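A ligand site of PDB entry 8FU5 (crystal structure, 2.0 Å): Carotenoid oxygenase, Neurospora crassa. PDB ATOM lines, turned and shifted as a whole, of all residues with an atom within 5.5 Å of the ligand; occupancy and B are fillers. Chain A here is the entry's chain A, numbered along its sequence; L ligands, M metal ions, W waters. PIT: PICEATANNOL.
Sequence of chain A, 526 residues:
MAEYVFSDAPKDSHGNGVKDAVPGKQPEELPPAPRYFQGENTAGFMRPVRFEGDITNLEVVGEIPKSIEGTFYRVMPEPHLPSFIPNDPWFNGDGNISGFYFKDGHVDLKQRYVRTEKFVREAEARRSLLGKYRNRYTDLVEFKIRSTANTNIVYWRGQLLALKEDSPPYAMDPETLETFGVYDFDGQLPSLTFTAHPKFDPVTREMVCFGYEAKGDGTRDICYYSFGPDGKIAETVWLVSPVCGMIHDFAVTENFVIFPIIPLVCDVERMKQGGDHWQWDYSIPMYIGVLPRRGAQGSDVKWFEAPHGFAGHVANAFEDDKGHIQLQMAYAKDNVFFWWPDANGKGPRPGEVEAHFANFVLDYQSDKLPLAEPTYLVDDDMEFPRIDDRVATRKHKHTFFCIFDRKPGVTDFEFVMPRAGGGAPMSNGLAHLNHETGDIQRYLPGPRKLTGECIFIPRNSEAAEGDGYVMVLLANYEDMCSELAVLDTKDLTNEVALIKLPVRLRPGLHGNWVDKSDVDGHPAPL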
ATOM      1  N   TRP A  90     -23.331   6.682  -3.527  1.00  0.00           N
ATOM      2  CA  TRP A  90     -24.119   5.468  -3.396  1.00  0.00           C
ATOM      3  C   TRP A  90     -24.776   5.381  -2.017  1.00  0.00           C
ATOM      4  O   TRP A  90     -25.942   5.024  -1.937  1.00  0.00           O
ATOM      5  CB  TRP A  90     -23.177   4.295  -3.685  1.00  0.00           C
ATOM      6  CG  TRP A  90     -23.777   2.928  -3.586  1.00  0.00           C
ATOM      7  CD1 TRP A  90     -24.895   2.446  -4.201  1.00  0.00           C
ATOM      8  CD2 TRP A  90     -23.207   1.821  -2.855  1.00  0.00           C
ATOM      9  NE1 TRP A  90     -25.059   1.122  -3.902  1.00  0.00           N
ATOM     10  CE2 TRP A  90     -24.047   0.714  -3.070  1.00  0.00           C
ATOM     11  CE3 TRP A  90     -22.075   1.681  -2.046  1.00  0.00           C
ATOM     12  CZ2 TRP A  90     -23.797  -0.524  -2.478  1.00  0.00           C
ATOM     13  CZ3 TRP A  90     -21.826   0.453  -1.474  1.00  0.00           C
ATOM     14  CH2 TRP A  90     -22.686  -0.634  -1.688  1.00  0.00           C
ATOM     15  N   PHE A  91     -24.042   5.761  -0.970  1.00  0.00           N
ATOM     16  CA  PHE A  91     -24.509   5.726   0.414  1.00  0.00           C
ATOM     17  C   PHE A  91     -25.695   6.651   0.689  1.00  0.00           C
ATOM     18  O   PHE A  91     -26.275   6.587   1.779  1.00  0.00           O
ATOM     19  CB  PHE A  91     -23.390   6.140   1.381  1.00  0.00           C
ATOM     20  CG  PHE A  91     -22.198   5.217   1.493  1.00  0.00           C
ATOM     21  CD1 PHE A  91     -22.183   3.932   0.935  1.00  0.00           C
ATOM     22  CD2 PHE A  91     -21.048   5.651   2.148  1.00  0.00           C
ATOM     23  CE1 PHE A  91     -21.078   3.112   1.054  1.00  0.00           C
ATOM     24  CE2 PHE A  91     -19.938   4.826   2.280  1.00  0.00           C
ATOM     25  CZ  PHE A  91     -19.946   3.558   1.730  1.00  0.00           C
ATOM     26  N   TYR A 133     -25.060  14.175   1.282  1.00  0.00           N
ATOM     27  CA  TYR A 133     -24.872  13.186   2.321  1.00  0.00           C
ATOM     28  C   TYR A 133     -24.556  13.883   3.646  1.00  0.00           C
ATOM     29  O   TYR A 133     -23.541  14.596   3.757  1.00  0.00           O
ATOM     30  CB  TYR A 133     -23.745  12.218   1.938  1.00  0.00           C
ATOM     31  CG  TYR A 133     -23.528  11.120   2.952  1.00  0.00           C
ATOM     32  CD1 TYR A 133     -24.408  10.043   3.033  1.00  0.00           C
ATOM     33  CD2 TYR A 133     -22.500  11.198   3.875  1.00  0.00           C
ATOM     34  CE1 TYR A 133     -24.249   9.057   3.987  1.00  0.00           C
ATOM     35  CE2 TYR A 133     -22.324  10.209   4.837  1.00  0.00           C
ATOM     36  CZ  TYR A 133     -23.205   9.142   4.897  1.00  0.00           C
ATOM     37  OH  TYR A 133     -23.044   8.178   5.852  1.00  0.00           O
ATOM     38  N   ASN A 150     -30.615   2.531   4.797  1.00  0.00           N
ATOM     39  CA  ASN A 150     -30.173   1.851   3.594  1.00  0.00           C
ATOM     40  C   ASN A 150     -28.943   0.969   3.815  1.00  0.00           C
ATOM     41  O   ASN A 150     -28.363   0.498   2.846  1.00  0.00           O
ATOM     42  CB  ASN A 150     -29.876   2.851   2.487  1.00  0.00           C
ATOM     43  CG  ASN A 150     -28.645   3.703   2.753  1.00  0.00           C
ATOM     44  OD1 ASN A 150     -28.018   3.625   3.811  1.00  0.00           O
ATOM     45  ND2 ASN A 150     -28.294   4.517   1.775  1.00  0.00           N
ATOM     46  N   THR A 151     -28.562   0.723   5.076  1.00  0.00           N
ATOM     47  CA  THR A 151     -27.244   0.146   5.337  1.00  0.00           C
ATOM     48  C   THR A 151     -27.333  -1.290   5.846  1.00  0.00           C
ATOM     49  O   THR A 151     -26.557  -2.148   5.423  1.00  0.00           O
ATOM     50  CB  THR A 151     -26.440   1.031   6.294  1.00  0.00           C
ATOM     51  OG1 THR A 151     -26.327   2.337   5.687  1.00  0.00           O
ATOM     52  CG2 THR A 151     -25.063   0.469   6.577  1.00  0.00           C
ATOM     53  N   LYS A 164     -29.375   2.969   9.739  1.00  0.00           N
ATOM     54  CA  LYS A 164     -28.573   4.019   9.118  1.00  0.00           C
ATOM     55  C   LYS A 164     -27.932   4.833  10.241  1.00  0.00           C
ATOM     56  O   LYS A 164     -28.632   5.342  11.112  1.00  0.00           O
ATOM     57  CB  LYS A 164     -29.460   4.865   8.201  1.00  0.00           C
ATOM     58  CG  LYS A 164     -28.768   6.028   7.510  1.00  0.00           C
ATOM     59  CD  LYS A 164     -27.706   5.609   6.551  1.00  0.00           C
ATOM     60  CE  LYS A 164     -27.225   6.754   5.681  1.00  0.00           C
ATOM     61  NZ  LYS A 164     -26.582   6.262   4.444  1.00  0.00           N
ATOM     62  N   GLU A 165     -26.604   4.942  10.216  1.00  0.00           N
ATOM     63  CA  GLU A 165     -25.814   5.304  11.389  1.00  0.00           C
ATOM     64  C   GLU A 165     -25.977   6.765  11.805  1.00  0.00           C
ATOM     65  O   GLU A 165     -25.449   7.137  12.849  1.00  0.00           O
ATOM     66  CB  GLU A 165     -24.333   4.953  11.160  1.00  0.00           C
ATOM     67  CG  GLU A 165     -23.637   5.773  10.083  1.00  0.00           C
ATOM     68  CD  GLU A 165     -22.375   5.101   9.566  1.00  0.00           C
ATOM     69  OE1 GLU A 165     -21.288   5.736   9.638  1.00  0.00           O
ATOM     70  OE2 GLU A 165     -22.470   3.923   9.126  1.00  0.00           O
ATOM     71  N   MET A 246     -15.607   8.907  12.009  1.00  0.00           N
ATOM     72  CA  MET A 246     -16.624   7.939  11.633  1.00  0.00           C
ATOM     73  C   MET A 246     -16.337   6.607  12.318  1.00  0.00           C
ATOM     74  O   MET A 246     -15.246   6.053  12.184  1.00  0.00           O
ATOM     75  CB  MET A 246     -16.650   7.742  10.103  1.00  0.00           C
ATOM     76  CG  MET A 246     -17.523   6.582   9.657  1.00  0.00           C
ATOM     77  SD  MET A 246     -17.391   6.231   7.876  1.00  0.00           S
ATOM     78  CE  MET A 246     -18.132   7.700   7.175  1.00  0.00           C
ATOM     79  N   HIS A 248     -17.996   3.307  11.942  1.00  0.00           N
ATOM     80  CA  HIS A 248     -18.971   2.578  11.134  1.00  0.00           C
ATOM     81  C   HIS A 248     -19.362   1.242  11.777  1.00  0.00           C
ATOM     82  O   HIS A 248     -20.522   0.829  11.690  1.00  0.00           O
ATOM     83  CB  HIS A 248     -18.428   2.337   9.717  1.00  0.00           C
ATOM     84  CG  HIS A 248     -19.385   1.537   8.896  1.00  0.00           C
ATOM     85  ND1 HIS A 248     -20.621   2.020   8.534  1.00  0.00           N
ATOM     86  CD2 HIS A 248     -19.307   0.289   8.409  1.00  0.00           C
ATOM     87  CE1 HIS A 248     -21.271   1.077   7.850  1.00  0.00           C
ATOM     88  NE2 HIS A 248     -20.491   0.018   7.754  1.00  0.00           N
ATOM     89  N   PHE A 310      -7.575   2.610   7.426  1.00  0.00           N
ATOM     90  CA  PHE A 310      -9.018   2.601   7.336  1.00  0.00           C
ATOM     91  C   PHE A 310      -9.565   1.378   8.079  1.00  0.00           C
ATOM     92  O   PHE A 310      -9.216   0.253   7.739  1.00  0.00           O
ATOM     93  CB  PHE A 310      -9.432   2.610   5.866  1.00  0.00           C
ATOM     94  CG  PHE A 310     -10.905   2.829   5.629  1.00  0.00           C
ATOM     95  CD1 PHE A 310     -11.802   1.783   5.763  1.00  0.00           C
ATOM     96  CD2 PHE A 310     -11.384   4.077   5.282  1.00  0.00           C
ATOM     97  CE1 PHE A 310     -13.153   1.990   5.542  1.00  0.00           C
ATOM     98  CE2 PHE A 310     -12.738   4.280   5.069  1.00  0.00           C
ATOM     99  CZ  PHE A 310     -13.613   3.235   5.203  1.00  0.00           C
ATOM    100  N   ALA A 311     -10.416   1.616   9.076  1.00  0.00           N
ATOM    101  CA  ALA A 311     -11.124   0.563   9.787  1.00  0.00           C
ATOM    102  C   ALA A 311     -12.292   0.071   8.941  1.00  0.00           C
ATOM    103  O   ALA A 311     -13.287   0.772   8.781  1.00  0.00           O
ATOM    104  CB  ALA A 311     -11.618   1.085  11.120  1.00  0.00           C
ATOM    105  N   GLY A 312     -12.144  -1.128   8.377  1.00  0.00           N
ATOM    106  CA  GLY A 312     -13.208  -1.809   7.646  1.00  0.00           C
ATOM    107  C   GLY A 312     -14.107  -2.630   8.580  1.00  0.00           C
ATOM    108  O   GLY A 312     -14.043  -2.464   9.790  1.00  0.00           O
ATOM    109  N   HIS A 313     -14.923  -3.510   8.004  1.00  0.00           N
ATOM    110  CA  HIS A 313     -15.906  -4.259   8.765  1.00  0.00           C
ATOM    111  C   HIS A 313     -15.240  -5.264   9.696  1.00  0.00           C
ATOM    112  O   HIS A 313     -14.244  -5.890   9.340  1.00  0.00           O
ATOM    113  CB  HIS A 313     -16.897  -4.960   7.819  1.00  0.00           C
ATOM    114  CG  HIS A 313     -17.838  -4.019   7.174  1.00  0.00           C
ATOM    115  ND1 HIS A 313     -17.808  -3.734   5.823  1.00  0.00           N
ATOM    116  CD2 HIS A 313     -18.813  -3.282   7.699  1.00  0.00           C
ATOM    117  CE1 HIS A 313     -18.757  -2.851   5.554  1.00  0.00           C
ATOM    118  NE2 HIS A 313     -19.382  -2.561   6.681  1.00  0.00           N
ATOM    119  N   VAL A 336     -10.390   4.283   1.875  1.00  0.00           N
ATOM    120  CA  VAL A 336     -11.285   3.493   1.040  1.00  0.00           C
ATOM    121  C   VAL A 336     -12.387   4.398   0.459  1.00  0.00           C
ATOM    122  O   VAL A 336     -12.804   4.181  -0.676  1.00  0.00           O
ATOM    123  CB  VAL A 336     -11.888   2.314   1.825  1.00  0.00           C
ATOM    124  CG1 VAL A 336     -12.969   1.590   1.042  1.00  0.00           C
ATOM    125  CG2 VAL A 336     -10.804   1.338   2.269  1.00  0.00           C
ATOM    126  N   PHE A 337     -12.831   5.391   1.231  1.00  0.00           N
ATOM    127  CA  PHE A 337     -13.862   6.311   0.774  1.00  0.00           C
ATOM    128  C   PHE A 337     -13.189   7.522   0.120  1.00  0.00           C
ATOM    129  O   PHE A 337     -13.259   8.651   0.628  1.00  0.00           O
ATOM    130  CB  PHE A 337     -14.793   6.692   1.932  1.00  0.00           C
ATOM    131  CG  PHE A 337     -15.538   5.567   2.604  1.00  0.00           C
ATOM    132  CD1 PHE A 337     -15.628   4.301   2.042  1.00  0.00           C
ATOM    133  CD2 PHE A 337     -16.135   5.773   3.849  1.00  0.00           C
ATOM    134  CE1 PHE A 337     -16.305   3.270   2.682  1.00  0.00           C
ATOM    135  CE2 PHE A 337     -16.830   4.745   4.482  1.00  0.00           C
ATOM    136  CZ  PHE A 337     -16.899   3.498   3.902  1.00  0.00           C
ATOM    137  N   GLU A 383     -13.351  -7.934   1.969  1.00  0.00           N
ATOM    138  CA  GLU A 383     -14.266  -7.162   2.814  1.00  0.00           C
ATOM    139  C   GLU A 383     -15.518  -8.001   3.084  1.00  0.00           C
ATOM    140  O   GLU A 383     -15.610  -9.157   2.644  1.00  0.00           O
ATOM    141  CB  GLU A 383     -14.598  -5.806   2.192  1.00  0.00           C
ATOM    142  CG  GLU A 383     -14.029  -4.611   2.944  1.00  0.00           C
ATOM    143  CD  GLU A 383     -14.706  -4.240   4.252  1.00  0.00           C
ATOM    144  OE1 GLU A 383     -15.725  -4.885   4.602  1.00  0.00           O
ATOM    145  OE2 GLU A 383     -14.232  -3.278   4.923  1.00  0.00           O
ATOM    146  N   PHE A 384     -16.456  -7.411   3.846  1.00  0.00           N
ATOM    147  CA  PHE A 384     -17.761  -7.981   4.121  1.00  0.00           C
ATOM    148  C   PHE A 384     -17.607  -9.368   4.743  1.00  0.00           C
ATOM    149  O   PHE A 384     -18.176 -10.348   4.247  1.00  0.00           O
ATOM    150  CB  PHE A 384     -18.625  -7.954   2.856  1.00  0.00           C
ATOM    151  CG  PHE A 384     -19.001  -6.559   2.435  1.00  0.00           C
ATOM    152  CD1 PHE A 384     -19.986  -5.846   3.112  1.00  0.00           C
ATOM    153  CD2 PHE A 384     -18.335  -5.932   1.397  1.00  0.00           C
ATOM    154  CE1 PHE A 384     -20.298  -4.548   2.747  1.00  0.00           C
ATOM    155  CE2 PHE A 384     -18.639  -4.627   1.039  1.00  0.00           C
ATOM    156  CZ  PHE A 384     -19.623  -3.941   1.704  1.00  0.00           C
ATOM    157  N   PRO A 425     -18.341  -0.795  -4.364  1.00  0.00           N
ATOM    158  CA  PRO A 425     -17.220  -1.723  -4.371  1.00  0.00           C
ATOM    159  C   PRO A 425     -17.511  -2.965  -5.208  1.00  0.00           C
ATOM    160  O   PRO A 425     -18.668  -3.272  -5.483  1.00  0.00           O
ATOM    161  CB  PRO A 425     -17.077  -2.102  -2.888  1.00  0.00           C
ATOM    162  CG  PRO A 425     -18.498  -2.022  -2.386  1.00  0.00           C
ATOM    163  CD  PRO A 425     -19.048  -0.782  -3.069  1.00  0.00           C
ATOM    164  N   LEU A 509     -25.929  -3.285   0.365  1.00  0.00           N
ATOM    165  CA  LEU A 509     -25.064  -3.318   1.520  1.00  0.00           C
ATOM    166  C   LEU A 509     -25.355  -4.593   2.310  1.00  0.00           C
ATOM    167  O   LEU A 509     -25.224  -5.681   1.742  1.00  0.00           O
ATOM    168  CB  LEU A 509     -25.230  -1.997   2.277  1.00  0.00           C
ATOM    169  CG  LEU A 509     -24.557  -0.804   1.590  1.00  0.00           C
ATOM    170  CD1 LEU A 509     -25.009   0.517   2.166  1.00  0.00           C
ATOM    171  CD2 LEU A 509     -23.038  -0.927   1.690  1.00  0.00           C
ATOM    172  N   HIS A 510     -25.765  -4.484   3.572  1.00  0.00           N
ATOM    173  CA  HIS A 510     -25.751  -5.633   4.455  1.00  0.00           C
ATOM    174  C   HIS A 510     -27.079  -6.388   4.405  1.00  0.00           C
ATOM    175  O   HIS A 510     -28.106  -5.852   3.974  1.00  0.00           O
ATOM    176  CB  HIS A 510     -25.369  -5.196   5.880  1.00  0.00           C
ATOM    177  CG  HIS A 510     -24.007  -4.603   5.954  1.00  0.00           C
ATOM    178  ND1 HIS A 510     -22.868  -5.375   5.872  1.00  0.00           N
ATOM    179  CD2 HIS A 510     -23.603  -3.329   6.067  1.00  0.00           C
ATOM    180  CE1 HIS A 510     -21.806  -4.570   5.953  1.00  0.00           C
ATOM    181  NE2 HIS A 510     -22.226  -3.330   6.074  1.00  0.00           N
HETATM  182  C1  PIT L   1     -16.687  -0.615   4.330  1.00  0.00           C
HETATM  183  C2  PIT L   1     -16.501  -1.136   3.058  1.00  0.00           C
HETATM  184  C3  PIT L   1     -17.477  -0.932   2.099  1.00  0.00           C
HETATM  185  C4  PIT L   1     -18.637  -0.236   2.399  1.00  0.00           C
HETATM  186  C5  PIT L   1     -18.824   0.294   3.675  1.00  0.00           C
HETATM  187  C6  PIT L   1     -17.839   0.099   4.642  1.00  0.00           C
HETATM  188  C7  PIT L   1     -20.039   1.066   3.973  1.00  0.00           C
HETATM  189  C8  PIT L   1     -20.140   1.996   4.924  1.00  0.00           C
HETATM  190  C9  PIT L   1     -21.202   3.002   5.080  1.00  0.00           C
HETATM  191  C10 PIT L   1     -22.412   2.910   4.389  1.00  0.00           C
HETATM  192  C11 PIT L   1     -23.386   3.883   4.533  1.00  0.00           C
HETATM  193  C12 PIT L   1     -23.139   5.008   5.331  1.00  0.00           C
HETATM  194  C13 PIT L   1     -21.924   5.135   5.969  1.00  0.00           C
HETATM  195  C14 PIT L   1     -20.966   4.147   5.833  1.00  0.00           C
HETATM  196  O1  PIT L   1     -24.095   5.978   5.483  1.00  0.00           O
HETATM  197  O2  PIT L   1     -17.341  -1.433   0.825  1.00  0.00           O
HETATM  198  O3  PIT L   1     -15.748  -0.777   5.315  1.00  0.00           O
HETATM  199  OAD PIT L   1     -24.583   3.744   3.874  1.00  0.00           O
HETATM  200 FE    FE M   1     -21.189  -1.664   6.977  1.00  0.00          FE
HETATM  201  O   HOH W   1     -15.976   0.131   8.102  1.00  0.00           O
HETATM  202  O   HOH W   2     -22.046  -0.364   5.460  1.00  0.00           O
HETATM  203  O   HOH W   3     -14.878  -2.227   0.176  1.00  0.00           O
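The side-chain hydroxyl (OH) of Tyr 133 is in hydrogen-bond range of an oxygen (O1) of the ligand, at 2.5 Å. The side-chain amide oxygen (OD1) of Asn 150 is in hydrogen-bond range of an oxygen (OAD) of the ligand (3.4 Å). An oxygen (O1) of the ligand lies within hydrogen-bond range of the side-chain amino group (NZ) of Lys 164 (2.7 Å). OE2 of Glu 383 lies within hydrogen-bond range of O3 of the ligand, at 3.0 Å. OG1 of Thr 151 lies within hydrogen-bond range of OAD of the ligand (2.9 Å).
The side-chain hydroxyl (OG1) of Thr 151 sits at hydrogen-bond distance from the side-chain amide oxygen (OD1) of Asn 150. NZ of Lys 164 lies within hydrogen-bond range of O of Phe 91 (2.7 Å). OD1 of Asn 150 is in hydrogen-bond range of NZ of Lys 164, 3.1 Å away. A ring nitrogen (ND1) of His 248 sits at hydrogen-bond distance from the side-chain carboxylate of Glu 165, at 2.7 Å. The backbone NH (N) of His 510 is in hydrogen-bond range of the backbone carbonyl oxygen (O) of Thr 151 (3.1 Å). The side-chain carboxylate (OE1) of Glu 383 lies within hydrogen-bond range of a ring nitrogen (ND1) of His 313 (2.7 Å). The side-chain amide nitrogen (ND2) of Asn 150 lies within hydrogen-bond range of the backbone carbonyl oxygen (O) of Phe 91, 2.9 Å away.
Water W1 lies within hydrogen-bond range of the backbone carbonyl oxygen of Ala 311 and an oxygen (O3) of the ligand.
Merely in contact with the ligand: Phe 91 (3.4 Å), Glu 165 (3.4 Å), His 248 (3.3 Å), Phe 310 (3.8 Å), Gly 312 (3.6 Å), His 313 (3.2 Å), Phe 337 (3.6 Å), Phe 384 (3.5 Å), Pro 425 (3.5 Å) and Leu 509 (3.7 Å). Hydrophobic or aromatic side chains that line the ligand: Phe 91, Tyr 133, His 248, Phe 310, His 313, Phe 337, Phe 384, Pro 425 and Leu 509. 15 residues have an atom within 4 Å of the ligand: Phe 91, Tyr 133, Asn 150, Thr 151, Lys 164, Glu 165, His 248, Phe 310, Gly 312, His 313, Phe 337, Glu 383, Phe 384, Pro 425 and Leu 509.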
